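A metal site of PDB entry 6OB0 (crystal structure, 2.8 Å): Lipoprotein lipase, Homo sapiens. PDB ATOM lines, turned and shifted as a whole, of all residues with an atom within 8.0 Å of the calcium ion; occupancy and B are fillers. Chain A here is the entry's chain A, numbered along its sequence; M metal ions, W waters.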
ATOM      1  N   LYS A 102       7.316  -7.736  29.912  1.00  0.00           N
ATOM      2  CA  LYS A 102       7.077  -8.222  31.270  1.00  0.00           C
ATOM      3  C   LYS A 102       5.606  -8.012  31.671  1.00  0.00           C
ATOM      4  O   LYS A 102       4.938  -8.952  32.070  1.00  0.00           O
ATOM      5  CB  LYS A 102       8.035  -7.532  32.278  1.00  0.00           C
ATOM      6  CG  LYS A 102       9.367  -8.251  32.493  1.00  0.00           C
ATOM      7  CD  LYS A 102       9.254  -9.453  33.456  1.00  0.00           C
ATOM      8  CE  LYS A 102      10.484 -10.336  33.530  1.00  0.00           C
ATOM      9  NZ  LYS A 102      10.235 -11.551  34.380  1.00  0.00           N
ATOM     10  N   ALA A 135       6.788 -12.798  20.978  1.00  0.00           N
ATOM     11  CA  ALA A 135       7.313 -14.151  21.266  1.00  0.00           C
ATOM     12  C   ALA A 135       7.835 -14.182  22.723  1.00  0.00           C
ATOM     13  O   ALA A 135       7.624 -15.159  23.423  1.00  0.00           O
ATOM     14  CB  ALA A 135       8.430 -14.510  20.275  1.00  0.00           C
ATOM     15  N   HIS A 136       8.441 -13.072  23.189  1.00  0.00           N
ATOM     16  CA  HIS A 136       8.928 -12.945  24.548  1.00  0.00           C
ATOM     17  C   HIS A 136       7.803 -12.645  25.527  1.00  0.00           C
ATOM     18  O   HIS A 136       7.804 -13.202  26.623  1.00  0.00           O
ATOM     19  CB  HIS A 136      10.071 -11.949  24.643  1.00  0.00           C
ATOM     20  CG  HIS A 136      11.224 -12.264  23.743  1.00  0.00           C
ATOM     21  ND1 HIS A 136      11.933 -13.457  23.867  1.00  0.00           N
ATOM     22  CD2 HIS A 136      11.756 -11.545  22.726  1.00  0.00           C
ATOM     23  CE1 HIS A 136      12.883 -13.407  22.942  1.00  0.00           C
ATOM     24  NE2 HIS A 136      12.819 -12.278  22.235  1.00  0.00           N
ATOM     25  N   ALA A 138       4.865 -13.856  25.129  1.00  0.00           N
ATOM     26  CA  ALA A 138       4.347 -15.223  25.219  1.00  0.00           C
ATOM     27  C   ALA A 138       5.166 -16.072  26.187  1.00  0.00           C
ATOM     28  O   ALA A 138       4.587 -16.795  26.998  1.00  0.00           O
ATOM     29  CB  ALA A 138       4.330 -15.859  23.855  1.00  0.00           C
ATOM     30  N   GLY A 139       6.485 -15.949  26.127  1.00  0.00           N
ATOM     31  CA  GLY A 139       7.409 -16.675  27.000  1.00  0.00           C
ATOM     32  C   GLY A 139       7.225 -16.300  28.460  1.00  0.00           C
ATOM     33  O   GLY A 139       7.111 -17.184  29.308  1.00  0.00           O
ATOM     34  N   ILE A 140       7.145 -15.002  28.733  1.00  0.00           N
ATOM     35  CA  ILE A 140       6.908 -14.506  30.082  1.00  0.00           C
ATOM     36  C   ILE A 140       5.511 -14.987  30.592  1.00  0.00           C
ATOM     37  O   ILE A 140       5.417 -15.463  31.717  1.00  0.00           O
ATOM     38  CB  ILE A 140       7.104 -12.967  30.128  1.00  0.00           C
ATOM     39  CG1 ILE A 140       8.608 -12.631  29.912  1.00  0.00           C
ATOM     40  CG2 ILE A 140       6.608 -12.345  31.428  1.00  0.00           C
ATOM     41  CD1 ILE A 140       8.881 -11.261  29.236  1.00  0.00           C
ATOM     42  N   ALA A 141       4.483 -14.932  29.735  1.00  0.00           N
ATOM     43  CA  ALA A 141       3.128 -15.374  30.039  1.00  0.00           C
ATOM     44  C   ALA A 141       3.143 -16.845  30.448  1.00  0.00           C
ATOM     45  O   ALA A 141       2.575 -17.193  31.488  1.00  0.00           O
ATOM     46  CB  ALA A 141       2.218 -15.169  28.837  1.00  0.00           C
ATOM     47  N   GLY A 142       3.819 -17.667  29.663  1.00  0.00           N
ATOM     48  CA  GLY A 142       3.955 -19.093  29.913  1.00  0.00           C
ATOM     49  C   GLY A 142       4.682 -19.392  31.216  1.00  0.00           C
ATOM     50  O   GLY A 142       4.295 -20.322  31.935  1.00  0.00           O
ATOM     51  N   SER A 143       5.708 -18.588  31.539  1.00  0.00           N
ATOM     52  CA  SER A 143       6.464 -18.755  32.766  1.00  0.00           C
ATOM     53  C   SER A 143       5.674 -18.291  34.013  1.00  0.00           C
ATOM     54  O   SER A 143       6.078 -18.596  35.133  1.00  0.00           O
ATOM     55  CB  SER A 143       7.804 -18.049  32.671  1.00  0.00           C
ATOM     56  OG  SER A 143       7.673 -16.637  32.706  1.00  0.00           O
ATOM     57  N   LEU A 144       4.542 -17.579  33.839  1.00  0.00           N
ATOM     58  CA  LEU A 144       3.714 -17.112  34.949  1.00  0.00           C
ATOM     59  C   LEU A 144       2.334 -17.829  35.096  1.00  0.00           C
ATOM     60  O   LEU A 144       1.578 -17.505  36.024  1.00  0.00           O
ATOM     61  CB  LEU A 144       3.531 -15.585  34.850  1.00  0.00           C
ATOM     62  CG  LEU A 144       4.748 -14.728  34.934  1.00  0.00           C
ATOM     63  CD1 LEU A 144       4.466 -13.330  34.410  1.00  0.00           C
ATOM     64  CD2 LEU A 144       5.288 -14.700  36.343  1.00  0.00           C
ATOM     65  N   ILE A 152       4.153 -23.058  22.555  1.00  0.00           N
ATOM     66  CA  ILE A 152       4.498 -21.690  22.226  1.00  0.00           C
ATOM     67  C   ILE A 152       5.279 -21.709  20.931  1.00  0.00           C
ATOM     68  O   ILE A 152       6.310 -22.369  20.851  1.00  0.00           O
ATOM     69  CB  ILE A 152       5.238 -20.851  23.315  1.00  0.00           C
ATOM     70  CG1 ILE A 152       4.439 -20.713  24.606  1.00  0.00           C
ATOM     71  CG2 ILE A 152       5.546 -19.464  22.766  1.00  0.00           C
ATOM     72  CD1 ILE A 152       5.283 -20.042  25.797  1.00  0.00           C
ATOM     73  N   GLU A 166      18.360 -13.298  30.380  1.00  0.00           N
ATOM     74  CA  GLU A 166      18.245 -14.596  31.033  1.00  0.00           C
ATOM     75  C   GLU A 166      16.860 -15.185  30.788  1.00  0.00           C
ATOM     76  O   GLU A 166      15.906 -14.429  30.579  1.00  0.00           O
ATOM     77  CB  GLU A 166      18.538 -14.454  32.540  1.00  0.00           C
ATOM     78  CG  GLU A 166      19.960 -14.857  32.907  1.00  0.00           C
ATOM     79  CD  GLU A 166      20.240 -16.347  33.041  1.00  0.00           C
ATOM     80  OE1 GLU A 166      19.625 -17.178  32.323  1.00  0.00           O
ATOM     81  OE2 GLU A 166      21.086 -16.689  33.901  1.00  0.00           O
ATOM     82  N   ALA A 167      16.735 -16.522  30.830  1.00  0.00           N
ATOM     83  CA  ALA A 167      15.474 -17.252  30.601  1.00  0.00           C
ATOM     84  C   ALA A 167      14.180 -16.588  31.174  1.00  0.00           C
ATOM     85  O   ALA A 167      13.194 -16.563  30.438  1.00  0.00           O
ATOM     86  CB  ALA A 167      15.602 -18.678  31.094  1.00  0.00           C
ATOM     87  N   PRO A 168      14.105 -16.032  32.416  1.00  0.00           N
ATOM     88  CA  PRO A 168      12.820 -15.443  32.864  1.00  0.00           C
ATOM     89  C   PRO A 168      12.377 -14.147  32.146  1.00  0.00           C
ATOM     90  O   PRO A 168      11.189 -13.814  32.197  1.00  0.00           O
ATOM     91  CB  PRO A 168      13.065 -15.160  34.348  1.00  0.00           C
ATOM     92  CG  PRO A 168      14.531 -14.922  34.440  1.00  0.00           C
ATOM     93  CD  PRO A 168      15.119 -15.939  33.485  1.00  0.00           C
ATOM     94  N   SER A 169      13.321 -13.420  31.499  1.00  0.00           N
ATOM     95  CA  SER A 169      13.046 -12.150  30.842  1.00  0.00           C
ATOM     96  C   SER A 169      12.753 -12.248  29.334  1.00  0.00           C
ATOM     97  O   SER A 169      12.342 -11.263  28.713  1.00  0.00           O
ATOM     98  CB  SER A 169      14.194 -11.176  31.094  1.00  0.00           C
ATOM     99  OG  SER A 169      14.353 -10.995  32.495  1.00  0.00           O
ATOM    100  N   ARG A 170      12.937 -13.432  28.771  1.00  0.00           N
ATOM    101  CA  ARG A 170      12.741 -13.715  27.351  1.00  0.00           C
ATOM    102  C   ARG A 170      12.087 -15.113  27.189  1.00  0.00           C
ATOM    103  O   ARG A 170      11.963 -15.853  28.174  1.00  0.00           O
ATOM    104  CB  ARG A 170      14.116 -13.745  26.653  1.00  0.00           C
ATOM    105  CG  ARG A 170      15.041 -14.855  27.178  1.00  0.00           C
ATOM    106  CD  ARG A 170      16.104 -15.231  26.177  1.00  0.00           C
ATOM    107  NE  ARG A 170      17.262 -15.849  26.825  1.00  0.00           N
ATOM    108  CZ  ARG A 170      17.406 -17.146  27.061  1.00  0.00           C
ATOM    109  NH1 ARG A 170      18.504 -17.589  27.665  1.00  0.00           N
ATOM    110  NH2 ARG A 170      16.455 -18.002  26.723  1.00  0.00           N
ATOM    111  N   LEU A 171      11.741 -15.484  25.921  1.00  0.00           N
ATOM    112  CA  LEU A 171      11.236 -16.808  25.610  1.00  0.00           C
ATOM    113  C   LEU A 171      12.382 -17.807  25.820  1.00  0.00           C
ATOM    114  O   LEU A 171      13.529 -17.486  25.489  1.00  0.00           O
ATOM    115  CB  LEU A 171      10.731 -16.852  24.155  1.00  0.00           C
ATOM    116  CG  LEU A 171      10.237 -18.188  23.620  1.00  0.00           C
ATOM    117  CD1 LEU A 171       8.909 -18.565  24.212  1.00  0.00           C
ATOM    118  CD2 LEU A 171      10.157 -18.138  22.132  1.00  0.00           C
ATOM    119  N   SER A 172      12.075 -18.960  26.430  1.00  0.00           N
ATOM    120  CA  SER A 172      13.009 -20.045  26.756  1.00  0.00           C
ATOM    121  C   SER A 172      12.223 -21.391  26.788  1.00  0.00           C
ATOM    122  O   SER A 172      10.994 -21.348  26.831  1.00  0.00           O
ATOM    123  CB  SER A 172      13.732 -19.757  28.082  1.00  0.00           C
ATOM    124  OG  SER A 172      12.909 -19.307  29.151  1.00  0.00           O
ATOM    125  N   PRO A 173      12.862 -22.583  26.713  1.00  0.00           N
ATOM    126  CA  PRO A 173      12.073 -23.838  26.630  1.00  0.00           C
ATOM    127  C   PRO A 173      11.242 -24.200  27.839  1.00  0.00           C
ATOM    128  O   PRO A 173      10.301 -24.977  27.717  1.00  0.00           O
ATOM    129  CB  PRO A 173      13.123 -24.906  26.329  1.00  0.00           C
ATOM    130  CG  PRO A 173      14.314 -24.170  25.858  1.00  0.00           C
ATOM    131  CD  PRO A 173      14.311 -22.879  26.588  1.00  0.00           C
ATOM    132  N   ASP A 174      11.553 -23.627  29.007  1.00  0.00           N
ATOM    133  CA  ASP A 174      10.797 -23.908  30.232  1.00  0.00           C
ATOM    134  C   ASP A 174       9.456 -23.189  30.261  1.00  0.00           C
ATOM    135  O   ASP A 174       8.644 -23.470  31.140  1.00  0.00           O
ATOM    136  CB  ASP A 174      11.623 -23.511  31.467  1.00  0.00           C
ATOM    137  CG  ASP A 174      11.916 -22.024  31.515  1.00  0.00           C
ATOM    138  OD1 ASP A 174      12.901 -21.588  30.847  1.00  0.00           O
ATOM    139  OD2 ASP A 174      11.158 -21.286  32.201  1.00  0.00           O
ATOM    140  N   ASP A 175       9.214 -22.257  29.317  1.00  0.00           N
ATOM    141  CA  ASP A 175       8.013 -21.444  29.276  1.00  0.00           C
ATOM    142  C   ASP A 175       6.740 -22.217  28.856  1.00  0.00           C
ATOM    143  O   ASP A 175       5.642 -21.733  29.145  1.00  0.00           O
ATOM    144  CB  ASP A 175       8.238 -20.200  28.411  1.00  0.00           C
ATOM    145  CG  ASP A 175       9.337 -19.286  28.936  1.00  0.00           C
ATOM    146  OD1 ASP A 175       9.652 -19.356  30.154  1.00  0.00           O
ATOM    147  OD2 ASP A 175       9.872 -18.499  28.147  1.00  0.00           O
ATOM    148  N   ALA A 176       6.858 -23.399  28.228  1.00  0.00           N
ATOM    149  CA  ALA A 176       5.700 -24.221  27.834  1.00  0.00           C
ATOM    150  C   ALA A 176       6.066 -25.676  27.773  1.00  0.00           C
ATOM    151  O   ALA A 176       7.246 -26.013  27.942  1.00  0.00           O
ATOM    152  CB  ALA A 176       5.156 -23.764  26.484  1.00  0.00           C
ATOM    153  N   VAL A 200      16.168 -20.707  21.445  1.00  0.00           N
ATOM    154  CA  VAL A 200      15.364 -20.399  22.644  1.00  0.00           C
ATOM    155  C   VAL A 200      14.212 -21.373  22.851  1.00  0.00           C
ATOM    156  O   VAL A 200      13.406 -21.164  23.755  1.00  0.00           O
ATOM    157  CB  VAL A 200      14.866 -18.927  22.689  1.00  0.00           C
ATOM    158  CG1 VAL A 200      16.034 -17.964  22.881  1.00  0.00           C
ATOM    159  CG2 VAL A 200      14.051 -18.559  21.464  1.00  0.00           C
HETATM  160 CA    CA M   1      11.346 -17.624  29.846  1.00  0.00          CA
HETATM  161  O   HOH W   1       9.879 -15.961  31.136  1.00  0.00           O
HETATM  162  O   HOH W   2      11.622 -18.516  31.789  1.00  0.00           O
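Within 4 Å of the calcium ion: Ala 167, Arg 170, Ser 172 and Asp 175. Along chain A the residues within 4 Å of the calcium ion span positions 167 to 175. The nearest printed residue that does not touch the calcium ion is Pro 168 (4.005 Å).
The calcium ion is bound by water W2. The calcium ion is bound by O of Ala 167 (2.2 Å). The calcium ion is bound by OG of Ser 172, 2.4 Å away. The side-chain carboxylate (OD2) of Asp 175 is bound to the calcium ion (2.4 Å). The calcium ion is bound by OD1 of Asp 175 (2.4 Å). O of Arg 170 is bound to the calcium ion, 2.5 Å away. Water W1 is bound to the calcium ion. The calcium ion has seven donor atoms within binding distance.
Water W1 lies within hydrogen-bond range of the backbone carbonyl oxygen (O) of Pro 168 (2.7 Å) and the side-chain hydroxyl (OG) of Ser 143 (2.8 Å).
OG of Ser 172 sits close to OD1 of Asp 174 (2.8 Å).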
